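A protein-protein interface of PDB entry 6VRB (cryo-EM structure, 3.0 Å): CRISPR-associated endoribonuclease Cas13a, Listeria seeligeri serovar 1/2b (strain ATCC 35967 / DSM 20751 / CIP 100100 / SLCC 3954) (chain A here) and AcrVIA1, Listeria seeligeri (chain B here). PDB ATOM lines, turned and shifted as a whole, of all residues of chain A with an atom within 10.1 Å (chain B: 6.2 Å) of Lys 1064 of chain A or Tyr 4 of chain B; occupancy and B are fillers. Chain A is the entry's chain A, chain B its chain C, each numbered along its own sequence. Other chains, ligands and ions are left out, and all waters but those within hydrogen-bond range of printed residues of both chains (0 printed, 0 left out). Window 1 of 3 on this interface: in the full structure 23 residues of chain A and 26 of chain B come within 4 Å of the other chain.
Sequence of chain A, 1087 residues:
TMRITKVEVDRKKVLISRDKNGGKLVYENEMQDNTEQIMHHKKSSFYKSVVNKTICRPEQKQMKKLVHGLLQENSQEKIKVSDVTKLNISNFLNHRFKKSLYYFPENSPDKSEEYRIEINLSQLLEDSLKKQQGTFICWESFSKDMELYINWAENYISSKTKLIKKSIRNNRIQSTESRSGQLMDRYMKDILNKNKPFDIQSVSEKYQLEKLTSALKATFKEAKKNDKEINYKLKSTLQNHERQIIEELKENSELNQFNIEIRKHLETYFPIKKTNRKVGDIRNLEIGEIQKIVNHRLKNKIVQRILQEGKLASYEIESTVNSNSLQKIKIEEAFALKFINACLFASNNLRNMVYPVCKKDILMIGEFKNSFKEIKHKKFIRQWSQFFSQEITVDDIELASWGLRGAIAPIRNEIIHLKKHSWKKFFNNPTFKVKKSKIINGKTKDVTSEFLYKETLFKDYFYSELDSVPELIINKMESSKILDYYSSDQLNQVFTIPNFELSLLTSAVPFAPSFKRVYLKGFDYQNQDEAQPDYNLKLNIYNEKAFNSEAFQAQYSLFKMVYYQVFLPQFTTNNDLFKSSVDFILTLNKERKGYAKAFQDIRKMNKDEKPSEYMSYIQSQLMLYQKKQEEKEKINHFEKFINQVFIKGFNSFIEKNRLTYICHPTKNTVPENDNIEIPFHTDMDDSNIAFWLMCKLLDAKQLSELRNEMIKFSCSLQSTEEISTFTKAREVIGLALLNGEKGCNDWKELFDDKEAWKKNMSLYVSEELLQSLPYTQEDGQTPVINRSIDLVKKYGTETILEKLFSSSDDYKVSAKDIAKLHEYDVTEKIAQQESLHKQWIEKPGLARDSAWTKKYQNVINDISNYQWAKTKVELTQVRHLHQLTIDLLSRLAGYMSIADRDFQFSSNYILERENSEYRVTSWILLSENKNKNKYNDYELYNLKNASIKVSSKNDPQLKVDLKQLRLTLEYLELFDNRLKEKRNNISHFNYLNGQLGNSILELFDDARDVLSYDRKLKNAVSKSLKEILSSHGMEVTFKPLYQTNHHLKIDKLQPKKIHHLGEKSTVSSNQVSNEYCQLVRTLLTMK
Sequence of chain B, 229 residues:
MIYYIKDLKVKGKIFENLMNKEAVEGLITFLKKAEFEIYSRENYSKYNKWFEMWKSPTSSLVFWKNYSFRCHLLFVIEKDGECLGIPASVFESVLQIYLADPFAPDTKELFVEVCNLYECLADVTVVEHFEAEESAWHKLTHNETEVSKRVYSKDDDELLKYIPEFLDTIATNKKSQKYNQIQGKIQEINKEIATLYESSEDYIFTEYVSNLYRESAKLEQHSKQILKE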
ATOM      1  N   TRP A 840     -18.857  11.901 -11.599  1.00  0.00           N
ATOM      2  CA  TRP A 840     -19.286  12.873 -10.609  1.00  0.00           C
ATOM      3  C   TRP A 840     -18.158  13.815 -10.199  1.00  0.00           C
ATOM      4  O   TRP A 840     -18.428  14.972  -9.859  1.00  0.00           O
ATOM      5  CB  TRP A 840     -19.865  12.145  -9.398  1.00  0.00           C
ATOM      6  CG  TRP A 840     -20.145  13.054  -8.283  1.00  0.00           C
ATOM      7  CD1 TRP A 840     -21.055  14.055  -8.252  1.00  0.00           C
ATOM      8  CD2 TRP A 840     -19.462  13.089  -7.034  1.00  0.00           C
ATOM      9  NE1 TRP A 840     -21.000  14.706  -7.048  1.00  0.00           N
ATOM     10  CE2 TRP A 840     -20.026  14.126  -6.282  1.00  0.00           C
ATOM     11  CE3 TRP A 840     -18.434  12.329  -6.474  1.00  0.00           C
ATOM     12  CZ2 TRP A 840     -19.596  14.429  -5.006  1.00  0.00           C
ATOM     13  CZ3 TRP A 840     -18.010  12.628  -5.214  1.00  0.00           C
ATOM     14  CH2 TRP A 840     -18.585  13.670  -4.489  1.00  0.00           C
ATOM     15  N   PRO A 844     -19.542  17.918 -10.586  1.00  0.00           N
ATOM     16  CA  PRO A 844     -20.207  17.739  -9.286  1.00  0.00           C
ATOM     17  C   PRO A 844     -21.653  18.191  -9.269  1.00  0.00           C
ATOM     18  O   PRO A 844     -22.372  17.848  -8.324  1.00  0.00           O
ATOM     19  CB  PRO A 844     -19.357  18.592  -8.336  1.00  0.00           C
ATOM     20  CG  PRO A 844     -18.058  18.748  -9.025  1.00  0.00           C
ATOM     21  CD  PRO A 844     -18.387  18.820 -10.479  1.00  0.00           C
ATOM     22  N   ALA A 847     -24.926  15.742  -8.862  1.00  0.00           N
ATOM     23  CA  ALA A 847     -25.582  15.432  -7.601  1.00  0.00           C
ATOM     24  C   ALA A 847     -26.937  16.104  -7.465  1.00  0.00           C
ATOM     25  O   ALA A 847     -27.826  15.551  -6.812  1.00  0.00           O
ATOM     26  CB  ALA A 847     -24.688  15.855  -6.440  1.00  0.00           C
ATOM     27  N   ARG A 848     -27.088  17.275  -8.095  1.00  0.00           N
ATOM     28  CA  ARG A 848     -28.352  18.059  -8.024  1.00  0.00           C
ATOM     29  C   ARG A 848     -29.253  17.732  -9.220  1.00  0.00           C
ATOM     30  O   ARG A 848     -30.154  18.539  -9.514  1.00  0.00           O
ATOM     31  CB  ARG A 848     -28.044  19.557  -7.938  1.00  0.00           C
ATOM     32  CG  ARG A 848     -27.698  20.032  -6.535  1.00  0.00           C
ATOM     33  CD  ARG A 848     -27.568  21.539  -6.457  1.00  0.00           C
ATOM     34  NE  ARG A 848     -26.359  21.970  -5.771  1.00  0.00           N
ATOM     35  CZ  ARG A 848     -25.163  21.418  -5.929  1.00  0.00           C
ATOM     36  NH1 ARG A 848     -25.004  20.398  -6.756  1.00  0.00           N
ATOM     37  NH2 ARG A 848     -24.126  21.886  -5.258  1.00  0.00           N
ATOM     38  N   THR A 853     -29.288  10.993  -9.906  1.00  0.00           N
ATOM     39  CA  THR A 853     -29.051  10.422  -8.551  1.00  0.00           C
ATOM     40  C   THR A 853     -30.020   9.265  -8.281  1.00  0.00           C
ATOM     41  O   THR A 853     -29.664   8.382  -7.482  1.00  0.00           O
ATOM     42  CB  THR A 853     -29.105  11.505  -7.468  1.00  0.00           C
ATOM     43  OG1 THR A 853     -30.372  12.155  -7.553  1.00  0.00           O
ATOM     44  CG2 THR A 853     -27.997  12.525  -7.605  1.00  0.00           C
ATOM     45  N   LYS A1057     -24.495   3.503   7.807  1.00  0.00           N
ATOM     46  CA  LYS A1057     -24.638   4.056   6.469  1.00  0.00           C
ATOM     47  C   LYS A1057     -23.323   4.630   5.956  1.00  0.00           C
ATOM     48  O   LYS A1057     -22.428   4.978   6.725  1.00  0.00           O
ATOM     49  CB  LYS A1057     -25.728   5.124   6.442  1.00  0.00           C
ATOM     50  CG  LYS A1057     -27.111   4.561   6.614  1.00  0.00           C
ATOM     51  CD  LYS A1057     -28.133   5.665   6.608  1.00  0.00           C
ATOM     52  CE  LYS A1057     -29.518   5.118   6.853  1.00  0.00           C
ATOM     53  NZ  LYS A1057     -30.528   6.205   6.890  1.00  0.00           N
ATOM     54  N   HIS A1059     -23.027   6.930   2.857  1.00  0.00           N
ATOM     55  CA  HIS A1059     -23.172   8.314   2.374  1.00  0.00           C
ATOM     56  C   HIS A1059     -22.258   8.601   1.178  1.00  0.00           C
ATOM     57  O   HIS A1059     -21.257   9.309   1.264  1.00  0.00           O
ATOM     58  CB  HIS A1059     -22.960   9.341   3.495  1.00  0.00           C
ATOM     59  CG  HIS A1059     -23.998   9.276   4.564  1.00  0.00           C
ATOM     60  ND1 HIS A1059     -25.278   9.751   4.385  1.00  0.00           N
ATOM     61  CD2 HIS A1059     -23.954   8.777   5.820  1.00  0.00           C
ATOM     62  CE1 HIS A1059     -25.976   9.550   5.485  1.00  0.00           C
ATOM     63  NE2 HIS A1059     -25.196   8.962   6.372  1.00  0.00           N
ATOM     64  N   HIS A1060     -22.625   7.982   0.062  1.00  0.00           N
ATOM     65  CA  HIS A1060     -21.968   8.201  -1.214  1.00  0.00           C
ATOM     66  C   HIS A1060     -22.209   9.619  -1.708  1.00  0.00           C
ATOM     67  O   HIS A1060     -23.166  10.287  -1.317  1.00  0.00           O
ATOM     68  CB  HIS A1060     -22.521   7.235  -2.253  1.00  0.00           C
ATOM     69  CG  HIS A1060     -22.485   5.810  -1.820  1.00  0.00           C
ATOM     70  ND1 HIS A1060     -21.421   4.975  -2.060  1.00  0.00           N
ATOM     71  CD2 HIS A1060     -23.366   5.099  -1.084  1.00  0.00           C
ATOM     72  CE1 HIS A1060     -21.672   3.792  -1.532  1.00  0.00           C
ATOM     73  NE2 HIS A1060     -22.841   3.844  -0.927  1.00  0.00           N
ATOM     74  N   LEU A1061     -21.297  10.063  -2.575  1.00  0.00           N
ATOM     75  CA  LEU A1061     -21.504  11.166  -3.514  1.00  0.00           C
ATOM     76  C   LEU A1061     -21.719  12.503  -2.801  1.00  0.00           C
ATOM     77  O   LEU A1061     -22.764  13.139  -2.896  1.00  0.00           O
ATOM     78  CB  LEU A1061     -22.644  10.791  -4.469  1.00  0.00           C
ATOM     79  CG  LEU A1061     -22.955  11.485  -5.778  1.00  0.00           C
ATOM     80  CD1 LEU A1061     -23.197  10.404  -6.765  1.00  0.00           C
ATOM     81  CD2 LEU A1061     -24.219  12.275  -5.651  1.00  0.00           C
ATOM     82  N   GLY A1062     -20.701  12.913  -2.065  1.00  0.00           N
ATOM     83  CA  GLY A1062     -20.651  14.241  -1.487  1.00  0.00           C
ATOM     84  C   GLY A1062     -20.917  14.238   0.006  1.00  0.00           C
ATOM     85  O   GLY A1062     -20.836  13.215   0.688  1.00  0.00           O
ATOM     86  N   GLU A1063     -21.250  15.425   0.513  1.00  0.00           N
ATOM     87  CA  GLU A1063     -21.415  15.642   1.945  1.00  0.00           C
ATOM     88  C   GLU A1063     -22.814  16.070   2.367  1.00  0.00           C
ATOM     89  O   GLU A1063     -23.212  15.784   3.497  1.00  0.00           O
ATOM     90  CB  GLU A1063     -20.402  16.682   2.443  1.00  0.00           C
ATOM     91  CG  GLU A1063     -20.557  18.070   1.848  1.00  0.00           C
ATOM     92  CD  GLU A1063     -19.503  19.038   2.344  1.00  0.00           C
ATOM     93  OE1 GLU A1063     -18.632  18.618   3.135  1.00  0.00           O
ATOM     94  OE2 GLU A1063     -19.543  20.220   1.942  1.00  0.00           O
ATOM     95  N   LYS A1064     -23.518  16.798   1.501  1.00  0.00           N
ATOM     96  CA  LYS A1064     -24.917  17.198   1.795  1.00  0.00           C
ATOM     97  C   LYS A1064     -25.788  16.373   0.849  1.00  0.00           C
ATOM     98  O   LYS A1064     -26.558  16.969   0.076  1.00  0.00           O
ATOM     99  CB  LYS A1064     -25.110  18.697   1.552  1.00  0.00           C
ATOM    100  CG  LYS A1064     -25.054  19.571   2.798  1.00  0.00           C
ATOM    101  CD  LYS A1064     -24.602  20.987   2.516  1.00  0.00           C
ATOM    102  CE  LYS A1064     -25.658  21.818   1.818  1.00  0.00           C
ATOM    103  NZ  LYS A1064     -25.412  23.270   1.981  1.00  0.00           N
ATOM    104  N   SER A1065     -25.655  15.045   0.918  1.00  0.00           N
ATOM    105  CA  SER A1065     -26.344  14.191  -0.029  1.00  0.00           C
ATOM    106  C   SER A1065     -27.235  13.191   0.688  1.00  0.00           C
ATOM    107  O   SER A1065     -27.081  12.939   1.884  1.00  0.00           O
ATOM    108  CB  SER A1065     -25.350  13.442  -0.911  1.00  0.00           C
ATOM    109  OG  SER A1065     -26.026  12.597  -1.820  1.00  0.00           O
ATOM    110  N   THR A1066     -28.170  12.622  -0.064  1.00  0.00           N
ATOM    111  CA  THR A1066     -29.091  11.629   0.456  1.00  0.00           C
ATOM    112  C   THR A1066     -28.878  10.245  -0.135  1.00  0.00           C
ATOM    113  O   THR A1066     -29.492   9.288   0.343  1.00  0.00           O
ATOM    114  CB  THR A1066     -30.533  12.077   0.206  1.00  0.00           C
ATOM    115  OG1 THR A1066     -30.719  12.331  -1.192  1.00  0.00           O
ATOM    116  CG2 THR A1066     -30.838  13.336   0.987  1.00  0.00           C
ATOM    117  N   VAL A1067     -28.038  10.116  -1.159  1.00  0.00           N
ATOM    118  CA  VAL A1067     -27.668   8.811  -1.690  1.00  0.00           C
ATOM    119  C   VAL A1067     -26.777   8.115  -0.673  1.00  0.00           C
ATOM    120  O   VAL A1067     -25.733   8.644  -0.278  1.00  0.00           O
ATOM    121  CB  VAL A1067     -26.962   8.951  -3.042  1.00  0.00           C
ATOM    122  CG1 VAL A1067     -26.439   7.617  -3.502  1.00  0.00           C
ATOM    123  CG2 VAL A1067     -27.912   9.509  -4.066  1.00  0.00           C
ATOM    124  N   SER A1068     -27.192   6.936  -0.230  1.00  0.00           N
ATOM    125  CA  SER A1068     -26.448   6.205   0.781  1.00  0.00           C
ATOM    126  C   SER A1068     -26.674   4.716   0.577  1.00  0.00           C
ATOM    127  O   SER A1068     -27.436   4.297  -0.295  1.00  0.00           O
ATOM    128  CB  SER A1068     -26.860   6.633   2.186  1.00  0.00           C
ATOM    129  OG  SER A1068     -28.184   6.228   2.464  1.00  0.00           O
ATOM    130  N   ILE B   2     -29.483  23.719  -1.844  1.00  0.00           N
ATOM    131  CA  ILE B   2     -29.407  22.342  -1.377  1.00  0.00           C
ATOM    132  C   ILE B   2     -30.188  22.271  -0.081  1.00  0.00           C
ATOM    133  O   ILE B   2     -29.788  22.875   0.919  1.00  0.00           O
ATOM    134  CB  ILE B   2     -27.963  21.872  -1.158  1.00  0.00           C
ATOM    135  CG1 ILE B   2     -27.186  21.903  -2.464  1.00  0.00           C
ATOM    136  CG2 ILE B   2     -27.956  20.466  -0.597  1.00  0.00           C
ATOM    137  CD1 ILE B   2     -25.711  21.701  -2.272  1.00  0.00           C
ATOM    138  N   TYR B   3     -31.293  21.545  -0.096  1.00  0.00           N
ATOM    139  CA  TYR B   3     -32.179  21.463   1.052  1.00  0.00           C
ATOM    140  C   TYR B   3     -31.770  20.268   1.898  1.00  0.00           C
ATOM    141  O   TYR B   3     -32.157  19.133   1.607  1.00  0.00           O
ATOM    142  CB  TYR B   3     -33.629  21.358   0.600  1.00  0.00           C
ATOM    143  CG  TYR B   3     -34.059  22.564  -0.186  1.00  0.00           C
ATOM    144  CD1 TYR B   3     -34.354  23.757   0.452  1.00  0.00           C
ATOM    145  CD2 TYR B   3     -34.164  22.512  -1.565  1.00  0.00           C
ATOM    146  CE1 TYR B   3     -34.740  24.865  -0.257  1.00  0.00           C
ATOM    147  CE2 TYR B   3     -34.555  23.617  -2.286  1.00  0.00           C
ATOM    148  CZ  TYR B   3     -34.841  24.792  -1.625  1.00  0.00           C
ATOM    149  OH  TYR B   3     -35.233  25.898  -2.342  1.00  0.00           O
ATOM    150  N   TYR B   4     -30.974  20.527   2.925  1.00  0.00           N
ATOM    151  CA  TYR B   4     -30.422  19.466   3.750  1.00  0.00           C
ATOM    152  C   TYR B   4     -30.160  20.061   5.121  1.00  0.00           C
ATOM    153  O   TYR B   4     -29.153  20.745   5.304  1.00  0.00           O
ATOM    154  CB  TYR B   4     -29.142  18.922   3.139  1.00  0.00           C
ATOM    155  CG  TYR B   4     -28.494  17.832   3.945  1.00  0.00           C
ATOM    156  CD1 TYR B   4     -28.970  16.532   3.897  1.00  0.00           C
ATOM    157  CD2 TYR B   4     -27.415  18.104   4.768  1.00  0.00           C
ATOM    158  CE1 TYR B   4     -28.384  15.537   4.638  1.00  0.00           C
ATOM    159  CE2 TYR B   4     -26.826  17.116   5.512  1.00  0.00           C
ATOM    160  CZ  TYR B   4     -27.312  15.836   5.444  1.00  0.00           C
ATOM    161  OH  TYR B   4     -26.724  14.845   6.185  1.00  0.00           O
ATOM    162  N   ILE B   5     -31.067  19.827   6.071  1.00  0.00           N
ATOM    163  CA  ILE B   5     -30.896  20.247   7.454  1.00  0.00           C
ATOM    164  C   ILE B   5     -31.110  18.985   8.281  1.00  0.00           C
ATOM    165  O   ILE B   5     -31.615  17.979   7.784  1.00  0.00           O
ATOM    166  CB  ILE B   5     -31.878  21.374   7.868  1.00  0.00           C
ATOM    167  CG1 ILE B   5     -32.005  22.430   6.779  1.00  0.00           C
ATOM    168  CG2 ILE B   5     -31.329  22.175   9.015  1.00  0.00           C
ATOM    169  CD1 ILE B   5     -33.121  23.416   6.996  1.00  0.00           C
ATOM    170  N   LYS B   6     -30.495  18.967   9.463  1.00  0.00           N
ATOM    171  CA  LYS B   6     -30.608  17.802  10.380  1.00  0.00           C
ATOM    172  C   LYS B   6     -31.936  17.896  11.136  1.00  0.00           C
ATOM    173  O   LYS B   6     -32.550  18.978  11.104  1.00  0.00           O
ATOM    174  CB  LYS B   6     -29.385  17.715  11.298  1.00  0.00           C
ATOM    175  CG  LYS B   6     -29.113  16.333  11.874  1.00  0.00           C
ATOM    176  CD  LYS B   6     -27.648  16.076  12.140  1.00  0.00           C
ATOM    177  CE  LYS B   6     -26.846  15.854  10.875  1.00  0.00           C
ATOM    178  NZ  LYS B   6     -27.121  14.525  10.279  1.00  0.00           N
ATOM    179  N   LEU B  18     -35.899  16.785   6.659  1.00  0.00           N
ATOM    180  CA  LEU B  18     -35.811  18.119   6.010  1.00  0.00           C
ATOM    181  C   LEU B  18     -34.778  18.032   4.885  1.00  0.00           C
ATOM    182  O   LEU B  18     -33.775  18.758   4.957  1.00  0.00           O
ATOM    183  CB  LEU B  18     -35.366  19.149   7.052  1.00  0.00           C
ATOM    184  CG  LEU B  18     -36.294  19.327   8.251  1.00  0.00           C
ATOM    185  CD1 LEU B  18     -35.589  20.074   9.372  1.00  0.00           C
ATOM    186  CD2 LEU B  18     -37.566  20.051   7.846  1.00  0.00           C
ATOM    187  N   MET B  19     -35.037  17.192   3.879  1.00  0.00           N
ATOM    188  CA  MET B  19     -34.107  17.052   2.726  1.00  0.00           C
ATOM    189  C   MET B  19     -34.821  17.387   1.412  1.00  0.00           C
ATOM    190  O   MET B  19     -34.340  16.937   0.359  1.00  0.00           O
ATOM    191  CB  MET B  19     -33.557  15.625   2.653  1.00  0.00           C
ATOM    192  CG  MET B  19     -33.108  15.090   3.995  1.00  0.00           C
ATOM    193  SD  MET B  19     -31.616  15.918   4.594  1.00  0.00           S
ATOM    194  CE  MET B  19     -31.307  14.989   6.095  1.00  0.00           C
ATOM    195  N   ASN B  20     -35.916  18.146   1.473  1.00  0.00           N
ATOM    196  CA  ASN B  20     -36.654  18.528   0.238  1.00  0.00           C
ATOM    197  C   ASN B  20     -37.016  20.016   0.305  1.00  0.00           C
ATOM    198  O   ASN B  20     -36.852  20.612   1.383  1.00  0.00           O
ATOM    199  CB  ASN B  20     -37.865  17.627  -0.014  1.00  0.00           C
ATOM    200  CG  ASN B  20     -39.054  17.971   0.854  1.00  0.00           C
ATOM    201  OD1 ASN B  20     -39.501  19.117   0.881  1.00  0.00           O
ATOM    202  ND2 ASN B  20     -39.577  16.987   1.565  1.00  0.00           N
ATOM    203  N   VAL B  24     -38.372  22.109   3.965  1.00  0.00           N
ATOM    204  CA  VAL B  24     -37.620  23.260   4.448  1.00  0.00           C
ATOM    205  C   VAL B  24     -38.511  24.488   4.509  1.00  0.00           C
ATOM    206  O   VAL B  24     -38.494  25.231   5.496  1.00  0.00           O
ATOM    207  CB  VAL B  24     -36.381  23.487   3.566  1.00  0.00           C
ATOM    208  CG1 VAL B  24     -35.680  24.775   3.936  1.00  0.00           C
ATOM    209  CG2 VAL B  24     -35.426  22.334   3.721  1.00  0.00           C
ATOM    210  N   ASP B 106     -23.784  10.420  13.460  1.00  0.00           N
ATOM    211  CA  ASP B 106     -23.556  11.195  12.251  1.00  0.00           C
ATOM    212  C   ASP B 106     -23.883  12.675  12.435  1.00  0.00           C
ATOM    213  O   ASP B 106     -24.193  13.362  11.457  1.00  0.00           O
ATOM    214  CB  ASP B 106     -24.369  10.599  11.102  1.00  0.00           C
ATOM    215  CG  ASP B 106     -23.953   9.174  10.780  1.00  0.00           C
ATOM    216  OD1 ASP B 106     -22.785   8.821  11.046  1.00  0.00           O
ATOM    217  OD2 ASP B 106     -24.793   8.405  10.261  1.00  0.00           O
ATOM    218  N   GLU B 113     -23.985  22.331  13.059  1.00  0.00           N
ATOM    219  CA  GLU B 113     -25.153  21.830  12.347  1.00  0.00           C
ATOM    220  C   GLU B 113     -26.135  22.921  11.957  1.00  0.00           C
ATOM    221  O   GLU B 113     -26.924  22.717  11.032  1.00  0.00           O
ATOM    222  CB  GLU B 113     -25.878  20.786  13.192  1.00  0.00           C
ATOM    223  CG  GLU B 113     -25.129  19.490  13.362  1.00  0.00           C
ATOM    224  CD  GLU B 113     -24.960  18.730  12.063  1.00  0.00           C
ATOM    225  OE1 GLU B 113     -25.818  18.852  11.166  1.00  0.00           O
ATOM    226  OE2 GLU B 113     -23.970  17.982  11.941  1.00  0.00           O
ATOM    227  N   ASN B 116     -26.593  24.790   8.199  1.00  0.00           N
ATOM    228  CA  ASN B 116     -27.480  24.332   7.143  1.00  0.00           C
ATOM    229  C   ASN B 116     -28.818  25.047   7.192  1.00  0.00           C
ATOM    230  O   ASN B 116     -29.386  25.370   6.143  1.00  0.00           O
ATOM    231  CB  ASN B 116     -27.676  22.831   7.273  1.00  0.00           C
ATOM    232  CG  ASN B 116     -26.407  22.063   7.024  1.00  0.00           C
ATOM    233  OD1 ASN B 116     -25.626  22.410   6.142  1.00  0.00           O
ATOM    234  ND2 ASN B 116     -26.195  21.004   7.793  1.00  0.00           N
ATOM    235  N   LEU B 117     -29.337  25.290   8.398  1.00  0.00           N
ATOM    236  CA  LEU B 117     -30.562  26.063   8.560  1.00  0.00           C
ATOM    237  C   LEU B 117     -30.367  27.507   8.126  1.00  0.00           C
ATOM    238  O   LEU B 117     -31.219  28.085   7.445  1.00  0.00           O
ATOM    239  CB  LEU B 117     -31.025  25.995  10.010  1.00  0.00           C
ATOM    240  CG  LEU B 117     -32.252  26.842  10.347  1.00  0.00           C
ATOM    241  CD1 LEU B 117     -33.442  26.392   9.545  1.00  0.00           C
ATOM    242  CD2 LEU B 117     -32.556  26.795  11.828  1.00  0.00           C
ATOM    243  N   GLU B 119     -28.213  28.851   6.020  1.00  0.00           N
ATOM    244  CA  GLU B 119     -28.037  29.042   4.589  1.00  0.00           C
ATOM    245  C   GLU B 119     -29.298  28.749   3.798  1.00  0.00           C
ATOM    246  O   GLU B 119     -29.292  28.896   2.575  1.00  0.00           O
ATOM    247  CB  GLU B 119     -26.888  28.177   4.078  1.00  0.00           C
ATOM    248  CG  GLU B 119     -25.532  28.677   4.511  1.00  0.00           C
ATOM    249  CD  GLU B 119     -24.412  27.758   4.097  1.00  0.00           C
ATOM    250  OE1 GLU B 119     -24.708  26.675   3.557  1.00  0.00           O
ATOM    251  OE2 GLU B 119     -23.238  28.112   4.327  1.00  0.00           O
ATOM    252  N   CYS B 120     -30.368  28.320   4.458  1.00  0.00           N
ATOM    253  CA  CYS B 120     -31.687  28.297   3.853  1.00  0.00           C
ATOM    254  C   CYS B 120     -32.532  29.486   4.278  1.00  0.00           C
ATOM    255  O   CYS B 120     -33.487  29.833   3.581  1.00  0.00           O
ATOM    256  CB  CYS B 120     -32.407  26.997   4.206  1.00  0.00           C
ATOM    257  SG  CYS B 120     -31.654  25.504   3.515  1.00  0.00           S
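Lys 1064 of chain A touches three residues of chain B. Of the printed residues of chain A, Tyr 4 of chain B touches Lys 1064 (3.4 Å). Of the printed residues of chain A, Glu 119 of chain B touches Lys 1064. Of the printed residues of chain B, Arg 848 of chain A touches Ile 2. Printed residues of chain B within 4 Å of His 1059 of chain A: Asp 106 (3.9 Å). Printed residues of chain B within 4 Å of Thr 1066 of chain A: Met 19. Pro 844 of chain A touches none of the printed residues of chain B. Leu 117 of chain B touches none of the printed residues of chain A. The nearest residue of chain B that does not touch Lys 1064 of chain A is Asn 116 of chain B (4.03 Å).
Among the printed residues, pairs that only touch across the chains: Arg 848 of chain A with Ile 2 of chain B, Lys 1064 of chain A with Tyr 4 of chain B, Lys 1064 of chain A with Ile 2 of chain B, Thr 1066 of chain A with Met 19 of chain B and His 1059 of chain A with Asp 106 of chain B.
The side-chain amino group of Lys 6 of chain B sits at hydrogen-bond distance from the backbone carbonyl oxygen of Asp 106 of chain B, 3.4 Å away.
OE1 of Glu 119 of chain B is in salt-bridge range of NZ of Lys 1064 of chain A (3.8 Å).
Hydrophobic or aromatic side chains of chain A within 4 Å of the printed part of chain B: His 1059. Among the printed residues, 6 pairs touch across the chains. Among the printed residues, Asp or Glu carboxylates within 4 Å of a Lys or Arg side-chain nitrogen of the other chain: Lys 1064 of chain A with Glu 119 of chain B.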
